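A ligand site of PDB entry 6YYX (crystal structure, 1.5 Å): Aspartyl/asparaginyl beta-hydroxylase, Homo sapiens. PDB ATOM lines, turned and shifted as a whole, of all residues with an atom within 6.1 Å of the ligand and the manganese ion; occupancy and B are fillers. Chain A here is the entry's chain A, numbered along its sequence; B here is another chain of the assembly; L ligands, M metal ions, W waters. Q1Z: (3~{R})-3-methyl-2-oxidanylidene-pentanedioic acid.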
ATOM      1  N   LEU A 290      34.194 -22.781  24.373  1.00  0.00           N
ATOM      2  CA  LEU A 290      34.138 -22.264  25.738  1.00  0.00           C
ATOM      3  C   LEU A 290      33.149 -22.970  26.645  1.00  0.00           C
ATOM      4  O   LEU A 290      33.034 -22.592  27.800  1.00  0.00           O
ATOM      5  CB  LEU A 290      33.793 -20.767  25.741  1.00  0.00           C
ATOM      6  CG  LEU A 290      34.755 -19.863  24.980  1.00  0.00           C
ATOM      7  CD1 LEU A 290      34.221 -18.466  24.955  1.00  0.00           C
ATOM      8  CD2 LEU A 290      36.119 -19.896  25.653  1.00  0.00           C
ATOM      9  N   TRP A 296      24.294 -22.668  24.449  1.00  0.00           N
ATOM     10  CA  TRP A 296      24.590 -21.240  24.532  1.00  0.00           C
ATOM     11  C   TRP A 296      24.681 -20.743  23.097  1.00  0.00           C
ATOM     12  O   TRP A 296      25.567 -21.205  22.351  1.00  0.00           O
ATOM     13  CB  TRP A 296      25.919 -21.003  25.278  1.00  0.00           C
ATOM     14  CG  TRP A 296      26.416 -19.613  25.306  1.00  0.00           C
ATOM     15  CD1 TRP A 296      25.710 -18.468  25.127  1.00  0.00           C
ATOM     16  CD2 TRP A 296      27.762 -19.235  25.547  1.00  0.00           C
ATOM     17  NE1 TRP A 296      26.544 -17.387  25.240  1.00  0.00           N
ATOM     18  CE2 TRP A 296      27.807 -17.829  25.514  1.00  0.00           C
ATOM     19  CE3 TRP A 296      28.931 -19.943  25.821  1.00  0.00           C
ATOM     20  CZ2 TRP A 296      28.990 -17.119  25.722  1.00  0.00           C
ATOM     21  CZ3 TRP A 296      30.079 -19.259  26.035  1.00  0.00           C
ATOM     22  CH2 TRP A 296      30.117 -17.859  25.972  1.00  0.00           C
ATOM     23  N   GLN A 298      24.173 -16.987  20.483  1.00  0.00           N
ATOM     24  CA  GLN A 298      24.233 -15.530  20.463  1.00  0.00           C
ATOM     25  C   GLN A 298      23.695 -15.014  19.146  1.00  0.00           C
ATOM     26  O   GLN A 298      23.965 -15.592  18.082  1.00  0.00           O
ATOM     27  CB  GLN A 298      25.689 -15.048  20.709  1.00  0.00           C
ATOM     28  CG  GLN A 298      26.186 -15.559  22.027  1.00  0.00           C
ATOM     29  CD  GLN A 298      27.433 -14.896  22.525  1.00  0.00           C
ATOM     30  OE1 GLN A 298      28.439 -14.800  21.819  1.00  0.00           O
ATOM     31  NE2 GLN A 298      27.376 -14.413  23.773  1.00  0.00           N
ATOM     32  N   SER A 339      22.289 -13.055  24.048  1.00  0.00           N
ATOM     33  CA  SER A 339      22.985 -14.236  24.517  1.00  0.00           C
ATOM     34  C   SER A 339      21.997 -15.084  25.291  1.00  0.00           C
ATOM     35  O   SER A 339      21.509 -14.644  26.350  1.00  0.00           O
ATOM     36  CB  SER A 339      24.166 -13.845  25.402  1.00  0.00           C
ATOM     37  OG  SER A 339      24.991 -14.971  25.617  1.00  0.00           O
ATOM     38  N   ILE A 340      21.653 -16.248  24.775  1.00  0.00           N
ATOM     39  CA  ILE A 340      20.705 -17.143  25.419  1.00  0.00           C
ATOM     40  C   ILE A 340      21.485 -18.341  25.927  1.00  0.00           C
ATOM     41  O   ILE A 340      22.361 -18.872  25.227  1.00  0.00           O
ATOM     42  CB  ILE A 340      19.575 -17.602  24.482  1.00  0.00           C
ATOM     43  CG1 ILE A 340      18.571 -18.409  25.306  1.00  0.00           C
ATOM     44  CG2 ILE A 340      20.126 -18.347  23.265  1.00  0.00           C
ATOM     45  CD1 ILE A 340      17.232 -18.308  24.740  1.00  0.00           C
ATOM     46  N   MET A 341      21.157 -18.780  27.138  1.00  0.00           N
ATOM     47  CA  MET A 341      21.792 -19.927  27.729  1.00  0.00           C
ATOM     48  C   MET A 341      20.749 -20.754  28.457  1.00  0.00           C
ATOM     49  O   MET A 341      19.887 -20.208  29.135  1.00  0.00           O
ATOM     50  CB  MET A 341      22.854 -19.493  28.712  1.00  0.00           C
ATOM     51  CG  MET A 341      23.717 -20.587  29.201  1.00  0.00           C
ATOM     52  SD  MET A 341      25.062 -19.964  30.231  1.00  0.00           S
ATOM     53  CE  MET A 341      25.955 -18.862  29.128  1.00  0.00           C
ATOM     54  N   VAL A 347      29.971 -22.705  31.322  1.00  0.00           N
ATOM     55  CA  VAL A 347      30.966 -22.051  30.491  1.00  0.00           C
ATOM     56  C   VAL A 347      32.291 -22.059  31.239  1.00  0.00           C
ATOM     57  O   VAL A 347      32.389 -21.593  32.384  1.00  0.00           O
ATOM     58  CB  VAL A 347      30.565 -20.612  30.168  1.00  0.00           C
ATOM     59  CG1 VAL A 347      31.671 -20.003  29.387  1.00  0.00           C
ATOM     60  CG2 VAL A 347      29.267 -20.571  29.428  1.00  0.00           C
ATOM     61  N   HIS A 350      37.366 -18.380  31.323  1.00  0.00           N
ATOM     62  CA  HIS A 350      38.054 -17.891  30.133  1.00  0.00           C
ATOM     63  C   HIS A 350      38.239 -16.386  30.233  1.00  0.00           C
ATOM     64  O   HIS A 350      37.656 -15.711  31.085  1.00  0.00           O
ATOM     65  CB  HIS A 350      37.287 -18.254  28.857  1.00  0.00           C
ATOM     66  CG  HIS A 350      35.969 -17.542  28.704  1.00  0.00           C
ATOM     67  ND1 HIS A 350      34.823 -17.934  29.366  1.00  0.00           N
ATOM     68  CD2 HIS A 350      35.632 -16.441  27.980  1.00  0.00           C
ATOM     69  CE1 HIS A 350      33.830 -17.114  29.031  1.00  0.00           C
ATOM     70  NE2 HIS A 350      34.292 -16.204  28.178  1.00  0.00           N
ATOM     71  N   THR A 351      39.060 -15.873  29.323  1.00  0.00           N
ATOM     72  CA  THR A 351      39.408 -14.478  29.203  1.00  0.00           C
ATOM     73  C   THR A 351      39.183 -14.038  27.756  1.00  0.00           C
ATOM     74  O   THR A 351      39.432 -14.813  26.830  1.00  0.00           O
ATOM     75  CB  THR A 351      40.881 -14.292  29.595  1.00  0.00           C
ATOM     76  OG1 THR A 351      41.067 -14.557  30.990  1.00  0.00           O
ATOM     77  CG2 THR A 351      41.289 -12.914  29.364  1.00  0.00           C
ATOM     78  N   GLY A 352      38.693 -12.815  27.574  1.00  0.00           N
ATOM     79  CA  GLY A 352      38.602 -12.245  26.256  1.00  0.00           C
ATOM     80  C   GLY A 352      39.952 -11.784  25.758  1.00  0.00           C
ATOM     81  O   GLY A 352      40.969 -11.846  26.483  1.00  0.00           O
ATOM     82  N   ARG A 359      32.463  -4.913  29.261  1.00  0.00           N
ATOM     83  CA  ARG A 359      31.305  -5.685  28.810  1.00  0.00           C
ATOM     84  C   ARG A 359      30.094  -5.385  29.700  1.00  0.00           C
ATOM     85  O   ARG A 359      30.124  -5.669  30.903  1.00  0.00           O
ATOM     86  CB  ARG A 359      31.630  -7.175  28.814  1.00  0.00           C
ATOM     87  CG  ARG A 359      30.537  -8.070  28.290  1.00  0.00           C
ATOM     88  CD  ARG A 359      31.167  -9.267  27.558  1.00  0.00           C
ATOM     89  NE  ARG A 359      31.595  -8.975  26.190  1.00  0.00           N
ATOM     90  CZ  ARG A 359      31.934  -9.901  25.325  1.00  0.00           C
ATOM     91  NH1 ARG A 359      31.918 -11.175  25.711  1.00  0.00           N
ATOM     92  NH2 ARG A 359      32.274  -9.588  24.086  1.00  0.00           N
ATOM     93  N   HIS A 361      26.126  -6.343  30.529  1.00  0.00           N
ATOM     94  CA  HIS A 361      25.056  -7.333  30.444  1.00  0.00           C
ATOM     95  C   HIS A 361      23.770  -6.710  30.957  1.00  0.00           C
ATOM     96  O   HIS A 361      23.713  -6.294  32.113  1.00  0.00           O
ATOM     97  CB  HIS A 361      25.356  -8.536  31.341  1.00  0.00           C
ATOM     98  CG  HIS A 361      26.331  -9.505  30.780  1.00  0.00           C
ATOM     99  ND1 HIS A 361      26.529 -10.732  31.357  1.00  0.00           N
ATOM    100  CD2 HIS A 361      27.155  -9.446  29.710  1.00  0.00           C
ATOM    101  CE1 HIS A 361      27.416 -11.405  30.657  1.00  0.00           C
ATOM    102  NE2 HIS A 361      27.827 -10.642  29.663  1.00  0.00           N
ATOM    103  N   ILE A 373      27.327 -15.608  37.496  1.00  0.00           N
ATOM    104  CA  ILE A 373      28.509 -15.240  36.748  1.00  0.00           C
ATOM    105  C   ILE A 373      29.575 -14.817  37.739  1.00  0.00           C
ATOM    106  O   ILE A 373      29.331 -13.995  38.629  1.00  0.00           O
ATOM    107  CB  ILE A 373      28.264 -14.103  35.726  1.00  0.00           C
ATOM    108  CG1 ILE A 373      29.606 -13.797  35.045  1.00  0.00           C
ATOM    109  CG2 ILE A 373      27.641 -12.923  36.381  1.00  0.00           C
ATOM    110  CD1 ILE A 373      29.534 -12.867  33.912  1.00  0.00           C
ATOM    111  N   TRP A 382      22.274 -11.851  37.636  1.00  0.00           N
ATOM    112  CA  TRP A 382      21.613 -10.879  36.769  1.00  0.00           C
ATOM    113  C   TRP A 382      20.263 -10.540  37.356  1.00  0.00           C
ATOM    114  O   TRP A 382      19.707 -11.283  38.181  1.00  0.00           O
ATOM    115  CB  TRP A 382      21.449 -11.445  35.359  1.00  0.00           C
ATOM    116  CG  TRP A 382      22.730 -11.717  34.611  1.00  0.00           C
ATOM    117  CD1 TRP A 382      23.439 -10.836  33.869  1.00  0.00           C
ATOM    118  CD2 TRP A 382      23.396 -12.957  34.509  1.00  0.00           C
ATOM    119  NE1 TRP A 382      24.526 -11.454  33.303  1.00  0.00           N
ATOM    120  CE2 TRP A 382      24.520 -12.770  33.701  1.00  0.00           C
ATOM    121  CE3 TRP A 382      23.144 -14.230  35.036  1.00  0.00           C
ATOM    122  CZ2 TRP A 382      25.390 -13.784  33.420  1.00  0.00           C
ATOM    123  CZ3 TRP A 382      24.013 -15.234  34.756  1.00  0.00           C
ATOM    124  CH2 TRP A 382      25.127 -15.012  33.977  1.00  0.00           C
ATOM    125  N   PHE A 390      31.320  -5.768  33.592  1.00  0.00           N
ATOM    126  CA  PHE A 390      32.586  -6.355  34.013  1.00  0.00           C
ATOM    127  C   PHE A 390      33.609  -6.216  32.914  1.00  0.00           C
ATOM    128  O   PHE A 390      33.307  -5.831  31.770  1.00  0.00           O
ATOM    129  CB  PHE A 390      32.444  -7.823  34.437  1.00  0.00           C
ATOM    130  CG  PHE A 390      32.011  -8.734  33.341  1.00  0.00           C
ATOM    131  CD1 PHE A 390      30.703  -8.704  32.862  1.00  0.00           C
ATOM    132  CD2 PHE A 390      32.925  -9.621  32.795  1.00  0.00           C
ATOM    133  CE1 PHE A 390      30.325  -9.563  31.863  1.00  0.00           C
ATOM    134  CE2 PHE A 390      32.582 -10.478  31.809  1.00  0.00           C
ATOM    135  CZ  PHE A 390      31.257 -10.462  31.342  1.00  0.00           C
ATOM    136  N   ASP A 392      35.934  -8.255  30.823  1.00  0.00           N
ATOM    137  CA  ASP A 392      36.034  -9.663  30.447  1.00  0.00           C
ATOM    138  C   ASP A 392      37.437 -10.075  30.045  1.00  0.00           C
ATOM    139  O   ASP A 392      37.638 -11.239  29.684  1.00  0.00           O
ATOM    140  CB  ASP A 392      35.013 -10.036  29.368  1.00  0.00           C
ATOM    141  CG  ASP A 392      35.472  -9.709  27.934  1.00  0.00           C
ATOM    142  OD1 ASP A 392      36.068  -8.647  27.720  1.00  0.00           O
ATOM    143  OD2 ASP A 392      35.141 -10.491  27.006  1.00  0.00           O
ATOM    144  N   HIS A 396      36.590 -15.186  33.794  1.00  0.00           N
ATOM    145  CA  HIS A 396      35.182 -15.240  34.180  1.00  0.00           C
ATOM    146  C   HIS A 396      34.595 -16.569  33.756  1.00  0.00           C
ATOM    147  O   HIS A 396      35.126 -17.278  32.881  1.00  0.00           O
ATOM    148  CB  HIS A 396      34.369 -14.057  33.606  1.00  0.00           C
ATOM    149  CG  HIS A 396      34.445 -13.889  32.113  1.00  0.00           C
ATOM    150  ND1 HIS A 396      35.533 -13.336  31.485  1.00  0.00           N
ATOM    151  CD2 HIS A 396      33.548 -14.162  31.140  1.00  0.00           C
ATOM    152  CE1 HIS A 396      35.319 -13.302  30.172  1.00  0.00           C
ATOM    153  NE2 HIS A 396      34.118 -13.797  29.943  1.00  0.00           N
ATOM    154  N   GLU A 397      33.479 -16.899  34.367  1.00  0.00           N
ATOM    155  CA  GLU A 397      32.904 -18.229  34.356  1.00  0.00           C
ATOM    156  C   GLU A 397      31.413 -18.063  34.572  1.00  0.00           C
ATOM    157  O   GLU A 397      31.014 -17.162  35.292  1.00  0.00           O
ATOM    158  CB  GLU A 397      33.518 -19.089  35.455  1.00  0.00           C
ATOM    159  CG  GLU A 397      33.174 -20.550  35.411  1.00  0.00           C
ATOM    160  CD  GLU A 397      33.920 -21.341  36.497  1.00  0.00           C
ATOM    161  OE1 GLU A 397      34.543 -20.710  37.375  1.00  0.00           O
ATOM    162  OE2 GLU A 397      33.824 -22.590  36.459  1.00  0.00           O
ATOM    163  N   VAL A 398      30.608 -18.915  33.929  1.00  0.00           N
ATOM    164  CA  VAL A 398      29.155 -18.811  34.045  1.00  0.00           C
ATOM    165  C   VAL A 398      28.537 -20.188  34.174  1.00  0.00           C
ATOM    166  O   VAL A 398      28.997 -21.147  33.545  1.00  0.00           O
ATOM    167  CB  VAL A 398      28.554 -18.083  32.822  1.00  0.00           C
ATOM    168  CG1 VAL A 398      27.069 -18.246  32.799  1.00  0.00           C
ATOM    169  CG2 VAL A 398      28.934 -16.633  32.835  1.00  0.00           C
ATOM    170  N   ARG A 406      17.521 -18.536  29.944  1.00  0.00           N
ATOM    171  CA  ARG A 406      18.045 -17.294  30.487  1.00  0.00           C
ATOM    172  C   ARG A 406      18.587 -16.452  29.346  1.00  0.00           C
ATOM    173  O   ARG A 406      19.523 -16.859  28.677  1.00  0.00           O
ATOM    174  CB  ARG A 406      19.165 -17.530  31.496  1.00  0.00           C
ATOM    175  CG  ARG A 406      19.718 -16.274  32.169  1.00  0.00           C
ATOM    176  CD  ARG A 406      21.240 -16.150  32.012  1.00  0.00           C
ATOM    177  NE  ARG A 406      21.647 -16.047  30.605  1.00  0.00           N
ATOM    178  CZ  ARG A 406      22.875 -15.891  30.141  1.00  0.00           C
ATOM    179  NH1 ARG A 406      23.924 -15.777  30.942  1.00  0.00           N
ATOM    180  NH2 ARG A 406      23.079 -15.816  28.823  1.00  0.00           N
ATOM    181  N   ILE A 408      20.037 -12.620  28.080  1.00  0.00           N
ATOM    182  CA  ILE A 408      20.624 -11.315  28.397  1.00  0.00           C
ATOM    183  C   ILE A 408      20.982 -10.631  27.075  1.00  0.00           C
ATOM    184  O   ILE A 408      20.946 -11.221  25.982  1.00  0.00           O
ATOM    185  CB  ILE A 408      21.865 -11.425  29.340  1.00  0.00           C
ATOM    186  CG1 ILE A 408      23.050 -12.023  28.586  1.00  0.00           C
ATOM    187  CG2 ILE A 408      21.500 -12.174  30.677  1.00  0.00           C
ATOM    188  CD1 ILE A 408      24.361 -12.136  29.335  1.00  0.00           C
ATOM    189  N   ILE A 410      24.095  -8.251  25.608  1.00  0.00           N
ATOM    190  CA  ILE A 410      25.494  -7.904  25.831  1.00  0.00           C
ATOM    191  C   ILE A 410      25.836  -6.684  24.984  1.00  0.00           C
ATOM    192  O   ILE A 410      25.692  -6.714  23.750  1.00  0.00           O
ATOM    193  CB  ILE A 410      26.437  -9.074  25.492  1.00  0.00           C
ATOM    194  CG1 ILE A 410      25.959 -10.312  26.277  1.00  0.00           C
ATOM    195  CG2 ILE A 410      27.870  -8.671  25.766  1.00  0.00           C
ATOM    196  CD1 ILE A 410      26.909 -11.554  26.280  1.00  0.00           C
ATOM    197  N   ASP B  18      34.747 -13.837  22.099  1.00  0.00           N
ATOM    198  CA  ASP B  18      34.795 -14.004  23.550  1.00  0.00           C
ATOM    199  C   ASP B  18      36.112 -14.568  24.065  1.00  0.00           C
ATOM    200  O   ASP B  18      36.378 -14.427  25.273  1.00  0.00           O
ATOM    201  CB  ASP B  18      33.667 -14.927  23.977  1.00  0.00           C
ATOM    202  CG  ASP B  18      32.453 -14.166  24.447  1.00  0.00           C
ATOM    203  OD1 ASP B  18      31.935 -13.305  23.676  1.00  0.00           O
ATOM    204  OD2 ASP B  18      32.049 -14.445  25.613  1.00  0.00           O
HETATM  205  C01 Q1Z L   1      30.507 -14.566  28.703  1.00  0.00           C
HETATM  206  C02 Q1Z L   1      29.117 -15.085  29.214  1.00  0.00           C
HETATM  207  C03 Q1Z L   1      27.845 -14.813  28.247  1.00  0.00           C
HETATM  208  C04 Q1Z L   1      29.298 -16.651  29.264  1.00  0.00           C
HETATM  209  C05 Q1Z L   1      30.599 -13.256  28.407  1.00  0.00           C
HETATM  210  C06 Q1Z L   1      26.535 -15.106  28.942  1.00  0.00           C
HETATM  211  O01 Q1Z L   1      31.502 -15.318  28.600  1.00  0.00           O
HETATM  212  O02 Q1Z L   1      31.694 -12.770  28.080  1.00  0.00           O
HETATM  213  O03 Q1Z L   1      29.608 -12.361  28.444  1.00  0.00           O
HETATM  214  O04 Q1Z L   1      25.644 -15.164  28.098  1.00  0.00           O
HETATM  215  O05 Q1Z L   1      26.451 -15.261  30.272  1.00  0.00           O
HETATM  216 MN    MN M   1      33.220 -14.270  28.022  1.00  0.00          MN
HETATM  217  O   HOH W   1      34.713 -13.188  26.984  1.00  0.00           O
HETATM  218  O   HOH W   2      29.609 -13.499  25.385  1.00  0.00           O
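NE2 of His 361 is in hydrogen-bond range of O03 of the ligand (2.8 Å). The side-chain hydroxyl (OG) of Ser 339 is in hydrogen-bond range of an oxygen (O04) of the ligand. O05 of the ligand is in salt-bridge range of NH1 of Arg 406. The guanidinium group (NH1) of Arg 359 is in salt-bridge range of an oxygen (O03) of the ligand, at 3.8 Å.
OD1 of Asp 18 of chain B lies within salt-bridge range of NH1 of Arg 359 (2.9 Å). NE1 of Trp 296 sits close to NE2 of Gln 298. O of Ile 408 is in hydrogen-bond range of N of Ser 339 (3.0 Å). The backbone carbonyl oxygen of Ser 339 is in hydrogen-bond range of the guanidinium group of Arg 406 (3.2 Å). The guanidinium group (NH1) of Arg 359 lies within salt-bridge range of the side-chain carboxylate (OD2) of Asp 392, 3.5 Å away. The backbone carbonyl oxygen (O) of Arg 406 lies within hydrogen-bond range of the backbone NH (N) of Met 341, at 3.0 Å. A ring nitrogen (ND1) of His 396 sits close to the backbone carbonyl oxygen (O) of Asp 392, at 3.5 Å. The side-chain hydroxyl (OG) of Ser 339 lies within hydrogen-bond range of the side-chain amide nitrogen (NE2) of Gln 298.
Residues that only touch the ligand: Ile 408, Ile 410, Trp 296, Val 398, Trp 382, Met 341, Phe 390 and Val 347. The nearest printed residue that does not touch the ligand is Asp 392 (4.3 Å).
Three residues have an atom within 4 Å of the manganese ion: His 350, His 396 and Asp 18 of chain B. The nearest printed residue that does not touch the manganese ion is Arg 359 (4.1 Å).
The manganese ion is bound by an oxygen (O01) of the ligand, water W1, an oxygen (O02) of the ligand, a ring nitrogen (NE2) of His 396, a ring nitrogen (NE2) of His 350 and the side-chain carboxylate (OD2) of Asp 18 of chain B.
Water W1 bridges O of Asp 18 of chain B (2.7 Å) and OD2 of Asp 392 (2.7 Å). Water W2 lies within hydrogen-bond range of OD1 of Asp 18 of chain B (2.9 Å), NE2 of Gln 298 (2.9 Å), O03 of the ligand (3.3 Å) and NH1 of Arg 359 (3.3 Å).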
